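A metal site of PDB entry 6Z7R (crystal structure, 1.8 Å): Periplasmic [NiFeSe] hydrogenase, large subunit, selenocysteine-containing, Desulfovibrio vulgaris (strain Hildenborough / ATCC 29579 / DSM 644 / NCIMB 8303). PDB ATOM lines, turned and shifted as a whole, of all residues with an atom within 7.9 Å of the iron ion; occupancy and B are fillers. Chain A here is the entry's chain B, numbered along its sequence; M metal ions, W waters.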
ATOM      1  N   TYR A  41      11.016 -10.066  -4.405  1.00  0.00           N
ATOM      2  CA  TYR A  41       9.940 -11.019  -4.691  1.00  0.00           C
ATOM      3  C   TYR A  41      10.385 -12.090  -5.676  1.00  0.00           C
ATOM      4  O   TYR A  41      11.072 -11.799  -6.664  1.00  0.00           O
ATOM      5  CB  TYR A  41       8.739 -10.274  -5.290  1.00  0.00           C
ATOM      6  CG  TYR A  41       7.611 -11.151  -5.734  1.00  0.00           C
ATOM      7  CD1 TYR A  41       6.641 -11.564  -4.834  1.00  0.00           C
ATOM      8  CD2 TYR A  41       7.459 -11.483  -7.066  1.00  0.00           C
ATOM      9  CE1 TYR A  41       5.553 -12.345  -5.249  1.00  0.00           C
ATOM     10  CE2 TYR A  41       6.397 -12.248  -7.502  1.00  0.00           C
ATOM     11  CZ  TYR A  41       5.448 -12.682  -6.601  1.00  0.00           C
ATOM     12  OH  TYR A  41       4.439 -13.452  -7.091  1.00  0.00           O
ATOM     13  N   GLU A  45       4.287 -18.934  -5.073  1.00  0.00           N
ATOM     14  CA  GLU A  45       2.924 -19.417  -5.110  1.00  0.00           C
ATOM     15  C   GLU A  45       2.432 -19.610  -6.539  1.00  0.00           C
ATOM     16  O   GLU A  45       1.530 -20.430  -6.778  1.00  0.00           O
ATOM     17  CB  GLU A  45       2.036 -18.432  -4.307  1.00  0.00           C
ATOM     18  CG  GLU A  45       2.367 -18.436  -2.809  1.00  0.00           C
ATOM     19  CD  GLU A  45       1.840 -17.236  -2.025  1.00  0.00           C
ATOM     20  OE1 GLU A  45       1.823 -16.124  -2.544  1.00  0.00           O
ATOM     21  OE2 GLU A  45       1.485 -17.384  -0.838  1.00  0.00           O
ATOM     22  N   GLU A 271      -5.546 -11.831   4.208  1.00  0.00           N
ATOM     23  CA  GLU A 271      -4.349 -11.131   3.767  1.00  0.00           C
ATOM     24  C   GLU A 271      -4.757  -9.890   2.968  1.00  0.00           C
ATOM     25  O   GLU A 271      -5.409 -10.006   1.929  1.00  0.00           O
ATOM     26  CB  GLU A 271      -3.438 -12.056   2.935  1.00  0.00           C
ATOM     27  CG  GLU A 271      -2.781 -13.145   3.751  1.00  0.00           C
ATOM     28  CD  GLU A 271      -1.672 -13.925   2.996  1.00  0.00           C
ATOM     29  OE1 GLU A 271      -1.979 -14.898   2.275  1.00  0.00           O
ATOM     30  OE2 GLU A 271      -0.483 -13.580   3.154  1.00  0.00           O
ATOM     31  N   PHE A 278       0.642  -5.910  -4.936  1.00  0.00           N
ATOM     32  CA  PHE A 278      -0.177  -6.929  -5.573  1.00  0.00           C
ATOM     33  C   PHE A 278      -1.460  -6.290  -6.092  1.00  0.00           C
ATOM     34  O   PHE A 278      -1.928  -5.290  -5.554  1.00  0.00           O
ATOM     35  CB  PHE A 278      -0.450  -8.104  -4.574  1.00  0.00           C
ATOM     36  CG  PHE A 278       0.820  -8.757  -4.079  1.00  0.00           C
ATOM     37  CD1 PHE A 278       1.423  -9.768  -4.835  1.00  0.00           C
ATOM     38  CD2 PHE A 278       1.443  -8.338  -2.938  1.00  0.00           C
ATOM     39  CE1 PHE A 278       2.594 -10.358  -4.418  1.00  0.00           C
ATOM     40  CE2 PHE A 278       2.658  -8.953  -2.506  1.00  0.00           C
ATOM     41  CZ  PHE A 278       3.217  -9.900  -3.267  1.00  0.00           C
ATOM     42  N   TYR A 287      -6.529 -17.679   3.081  1.00  0.00           N
ATOM     43  CA  TYR A 287      -5.506 -18.428   2.362  1.00  0.00           C
ATOM     44  C   TYR A 287      -6.098 -19.499   1.434  1.00  0.00           C
ATOM     45  O   TYR A 287      -5.486 -19.823   0.415  1.00  0.00           O
ATOM     46  CB  TYR A 287      -4.513 -19.063   3.379  1.00  0.00           C
ATOM     47  CG  TYR A 287      -5.126 -19.965   4.435  1.00  0.00           C
ATOM     48  CD1 TYR A 287      -5.350 -21.301   4.197  1.00  0.00           C
ATOM     49  CD2 TYR A 287      -5.515 -19.465   5.682  1.00  0.00           C
ATOM     50  CE1 TYR A 287      -5.951 -22.136   5.164  1.00  0.00           C
ATOM     51  CE2 TYR A 287      -6.110 -20.275   6.634  1.00  0.00           C
ATOM     52  CZ  TYR A 287      -6.318 -21.596   6.376  1.00  0.00           C
ATOM     53  OH  TYR A 287      -6.899 -22.372   7.356  1.00  0.00           O
ATOM     54  N   LYS A 291      -4.636 -15.481  -3.784  1.00  0.00           N
ATOM     55  CA  LYS A 291      -4.160 -15.304  -5.144  1.00  0.00           C
ATOM     56  C   LYS A 291      -2.931 -14.420  -5.054  1.00  0.00           C
ATOM     57  O   LYS A 291      -2.904 -13.471  -4.255  1.00  0.00           O
ATOM     58  CB  LYS A 291      -5.210 -14.624  -6.064  1.00  0.00           C
ATOM     59  CG  LYS A 291      -6.524 -15.362  -6.192  1.00  0.00           C
ATOM     60  CD  LYS A 291      -7.468 -14.654  -7.135  1.00  0.00           C
ATOM     61  CE  LYS A 291      -8.780 -15.415  -7.259  1.00  0.00           C
ATOM     62  NZ  LYS A 291      -9.892 -14.450  -7.455  1.00  0.00           N
ATOM     63  N   THR A 292      -1.947 -14.666  -5.900  1.00  0.00           N
ATOM     64  CA  THR A 292      -0.760 -13.843  -5.893  1.00  0.00           C
ATOM     65  C   THR A 292      -0.546 -13.272  -7.293  1.00  0.00           C
ATOM     66  O   THR A 292      -0.016 -13.931  -8.190  1.00  0.00           O
ATOM     67  CB  THR A 292       0.430 -14.659  -5.375  1.00  0.00           C
ATOM     68  OG1 THR A 292       0.083 -15.246  -4.102  1.00  0.00           O
ATOM     69  CG2 THR A 292       1.624 -13.741  -5.184  1.00  0.00           C
ATOM     70  N   PHE A 304       6.538  -5.846  -0.752  1.00  0.00           N
ATOM     71  CA  PHE A 304       6.133  -7.124  -1.308  1.00  0.00           C
ATOM     72  C   PHE A 304       5.521  -8.065  -0.264  1.00  0.00           C
ATOM     73  O   PHE A 304       5.070  -9.160  -0.623  1.00  0.00           O
ATOM     74  CB  PHE A 304       7.318  -7.806  -2.008  1.00  0.00           C
ATOM     75  CG  PHE A 304       7.624  -7.210  -3.344  1.00  0.00           C
ATOM     76  CD1 PHE A 304       6.717  -7.278  -4.375  1.00  0.00           C
ATOM     77  CD2 PHE A 304       8.813  -6.602  -3.567  1.00  0.00           C
ATOM     78  CE1 PHE A 304       6.981  -6.741  -5.614  1.00  0.00           C
ATOM     79  CE2 PHE A 304       9.093  -6.040  -4.824  1.00  0.00           C
ATOM     80  CZ  PHE A 304       8.170  -6.123  -5.834  1.00  0.00           C
ATOM     81  N   LYS A 306       2.568  -9.113   2.015  1.00  0.00           N
ATOM     82  CA  LYS A 306       1.167  -8.879   2.271  1.00  0.00           C
ATOM     83  C   LYS A 306       0.953  -8.584   3.766  1.00  0.00           C
ATOM     84  O   LYS A 306       1.856  -8.738   4.587  1.00  0.00           O
ATOM     85  CB  LYS A 306       0.324 -10.103   1.844  1.00  0.00           C
ATOM     86  CG  LYS A 306       0.393 -10.424   0.327  1.00  0.00           C
ATOM     87  CD  LYS A 306      -0.598 -11.520  -0.037  1.00  0.00           C
ATOM     88  CE  LYS A 306      -0.447 -11.969  -1.468  1.00  0.00           C
ATOM     89  NZ  LYS A 306      -1.081 -13.332  -1.731  1.00  0.00           N
ATOM     90  N   LEU A 415       1.719 -21.549   7.956  1.00  0.00           N
ATOM     91  CA  LEU A 415       0.826 -22.505   7.318  1.00  0.00           C
ATOM     92  C   LEU A 415       1.082 -22.488   5.818  1.00  0.00           C
ATOM     93  O   LEU A 415       1.433 -21.439   5.233  1.00  0.00           O
ATOM     94  CB  LEU A 415      -0.666 -22.235   7.591  1.00  0.00           C
ATOM     95  CG  LEU A 415      -1.333 -21.020   6.991  1.00  0.00           C
ATOM     96  CD1 LEU A 415      -1.848 -21.309   5.572  1.00  0.00           C
ATOM     97  CD2 LEU A 415      -2.492 -20.599   7.877  1.00  0.00           C
ATOM     98  N   TYR A 428      -1.302 -23.011  -4.328  1.00  0.00           N
ATOM     99  CA  TYR A 428      -0.485 -23.227  -3.139  1.00  0.00           C
ATOM    100  C   TYR A 428      -0.328 -21.853  -2.520  1.00  0.00           C
ATOM    101  O   TYR A 428       0.128 -20.937  -3.183  1.00  0.00           O
ATOM    102  CB  TYR A 428       0.861 -23.852  -3.484  1.00  0.00           C
ATOM    103  CG  TYR A 428       1.542 -24.600  -2.365  1.00  0.00           C
ATOM    104  CD1 TYR A 428       2.072 -23.928  -1.274  1.00  0.00           C
ATOM    105  CD2 TYR A 428       1.734 -25.961  -2.435  1.00  0.00           C
ATOM    106  CE1 TYR A 428       2.723 -24.608  -0.247  1.00  0.00           C
ATOM    107  CE2 TYR A 428       2.396 -26.651  -1.412  1.00  0.00           C
ATOM    108  CZ  TYR A 428       2.904 -25.977  -0.327  1.00  0.00           C
ATOM    109  OH  TYR A 428       3.550 -26.679   0.663  1.00  0.00           O
ATOM    110  N   GLN A 429      -0.741 -21.695  -1.279  1.00  0.00           N
ATOM    111  CA  GLN A 429      -0.639 -20.422  -0.593  1.00  0.00           C
ATOM    112  C   GLN A 429       0.163 -20.594   0.696  1.00  0.00           C
ATOM    113  O   GLN A 429      -0.043 -21.571   1.432  1.00  0.00           O
ATOM    114  CB  GLN A 429      -2.036 -19.791  -0.311  1.00  0.00           C
ATOM    115  CG  GLN A 429      -2.740 -19.301  -1.582  1.00  0.00           C
ATOM    116  CD  GLN A 429      -2.069 -18.086  -2.202  1.00  0.00           C
ATOM    117  OE1 GLN A 429      -1.663 -17.147  -1.508  1.00  0.00           O
ATOM    118  NE2 GLN A 429      -1.919 -18.111  -3.514  1.00  0.00           N
ATOM    119  N   ILE A 430       1.070 -19.651   0.937  1.00  0.00           N
ATOM    120  CA  ILE A 430       1.943 -19.643   2.105  1.00  0.00           C
ATOM    121  C   ILE A 430       1.634 -18.425   2.979  1.00  0.00           C
ATOM    122  O   ILE A 430       1.579 -17.280   2.488  1.00  0.00           O
ATOM    123  CB  ILE A 430       3.405 -19.619   1.635  1.00  0.00           C
ATOM    124  CG1 ILE A 430       3.720 -20.903   0.889  1.00  0.00           C
ATOM    125  CG2 ILE A 430       4.419 -19.493   2.830  1.00  0.00           C
ATOM    126  CD1 ILE A 430       4.513 -20.662  -0.439  1.00  0.00           C
ATOM    127  N   VAL A 431       1.445 -18.666   4.277  1.00  0.00           N
ATOM    128  CA  VAL A 431       1.324 -17.634   5.297  1.00  0.00           C
ATOM    129  C   VAL A 431       2.377 -17.937   6.354  1.00  0.00           C
ATOM    130  O   VAL A 431       2.233 -18.887   7.107  1.00  0.00           O
ATOM    131  CB  VAL A 431      -0.088 -17.583   5.905  1.00  0.00           C
ATOM    132  CG1 VAL A 431      -0.200 -16.464   6.947  1.00  0.00           C
ATOM    133  CG2 VAL A 431      -1.121 -17.365   4.820  1.00  0.00           C
ATOM    134  N   SER A 432       3.440 -17.126   6.402  1.00  0.00           N
ATOM    135  CA  SER A 432       4.664 -17.387   7.164  1.00  0.00           C
ATOM    136  C   SER A 432       4.888 -16.428   8.341  1.00  0.00           C
ATOM    137  O   SER A 432       4.213 -15.409   8.511  1.00  0.00           O
ATOM    138  CB  SER A 432       5.836 -17.293   6.220  1.00  0.00           C
ATOM    139  OG  SER A 432       5.983 -15.962   5.774  1.00  0.00           O
ATOM    140  N   LEU A 435       5.911 -12.820   7.787  1.00  0.00           N
ATOM    141  CA  LEU A 435       4.785 -12.118   7.194  1.00  0.00           C
ATOM    142  C   LEU A 435       3.936 -11.484   8.291  1.00  0.00           C
ATOM    143  O   LEU A 435       3.592 -10.305   8.191  1.00  0.00           O
ATOM    144  CB  LEU A 435       3.988 -13.097   6.341  1.00  0.00           C
ATOM    145  CG  LEU A 435       2.654 -12.744   5.731  1.00  0.00           C
ATOM    146  CD1 LEU A 435       2.768 -11.900   4.542  1.00  0.00           C
ATOM    147  CD2 LEU A 435       2.075 -14.106   5.321  1.00  0.00           C
ATOM    148  N   CYS A 481      11.098 -15.481   3.773  1.00  0.00           N
ATOM    149  CA  CYS A 481       9.847 -16.073   4.233  1.00  0.00           C
ATOM    150  C   CYS A 481       8.691 -15.104   4.132  1.00  0.00           C
ATOM    151  O   CYS A 481       7.547 -15.545   3.907  1.00  0.00           O
ATOM    152  CB  CYS A 481       9.962 -16.485   5.700  1.00  0.00           C
ATOM    153  SG  CYS A 481      10.796 -18.032   5.933  1.00  0.00           S
ATOM    154  N   ALA A 482       8.929 -13.801   4.378  1.00  0.00           N
ATOM    155  CA  ALA A 482       7.791 -12.856   4.435  1.00  0.00           C
ATOM    156  C   ALA A 482       7.155 -12.678   3.054  1.00  0.00           C
ATOM    157  O   ALA A 482       5.930 -12.596   2.928  1.00  0.00           O
ATOM    158  CB  ALA A 482       8.191 -11.499   5.047  1.00  0.00           C
ATOM    159  N   VAL A 483       7.965 -12.617   2.000  1.00  0.00           N
ATOM    160  CA  VAL A 483       7.464 -12.366   0.655  1.00  0.00           C
ATOM    161  C   VAL A 483       7.259 -13.670  -0.105  1.00  0.00           C
ATOM    162  O   VAL A 483       6.308 -13.799  -0.880  1.00  0.00           O
ATOM    163  CB  VAL A 483       8.413 -11.449  -0.153  1.00  0.00           C
ATOM    164  CG1 VAL A 483       7.835 -11.255  -1.552  1.00  0.00           C
ATOM    165  CG2 VAL A 483       8.671 -10.137   0.504  1.00  0.00           C
ATOM    166  N   HIS A 484       8.179 -14.603   0.051  1.00  0.00           N
ATOM    167  CA  HIS A 484       8.286 -15.775  -0.804  1.00  0.00           C
ATOM    168  C   HIS A 484       8.021 -15.481  -2.297  1.00  0.00           C
ATOM    169  O   HIS A 484       8.644 -14.609  -2.951  1.00  0.00           O
ATOM    170  CB  HIS A 484       7.356 -16.917  -0.305  1.00  0.00           C
ATOM    171  CG  HIS A 484       6.056 -16.483   0.241  1.00  0.00           C
ATOM    172  ND1 HIS A 484       5.919 -16.024   1.525  1.00  0.00           N
ATOM    173  CD2 HIS A 484       4.808 -16.528  -0.285  1.00  0.00           C
ATOM    174  CE1 HIS A 484       4.652 -15.749   1.746  1.00  0.00           C
ATOM    175  NE2 HIS A 484       3.953 -16.053   0.674  1.00  0.00           N
ATOM    176  OXT HIS A 484       7.194 -16.181  -2.886  1.00  0.00           O
HETATM  177 FE    FE M   1       1.840 -15.852   0.738  1.00  0.00          FE
HETATM  178  O   HOH W   1       1.716 -14.136   2.245  1.00  0.00           O
HETATM  179  O   HOH W   2      -0.367 -15.771   0.639  1.00  0.00           O
HETATM  180  O   HOH W   3       1.915 -14.377  -1.069  1.00  0.00           O
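The iron ion is bound by a ring nitrogen (NE2) of His 484, water W2, the side-chain carboxylate (OE2) of Glu 45, the backbone carbonyl oxygen (O) of Ile 430, water W1 and water W3.
A ring nitrogen (ND1) of His 484 sits at hydrogen-bond distance from the backbone carbonyl oxygen (O) of Cys 481, at 2.9 Å.
The side-chain carboxylate (OE2) of Glu 45 sits close to the side-chain amide oxygen (OE1) of Gln 429 (3.2 Å).
OE1 of Glu 45 lies within hydrogen-bond range of OG1 of Thr 292 (2.5 Å).
Of the 20 residues printed, 3 come within 4 Å of the iron ion.
Water W2 lies within hydrogen-bond range of the side-chain carboxylate (OE1) of Glu 271 (2.5 Å), the side-chain amide oxygen (OE1) of Gln 429 (2.9 Å) and the side-chain amino group (NZ) of Lys 306 (3.5 Å).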
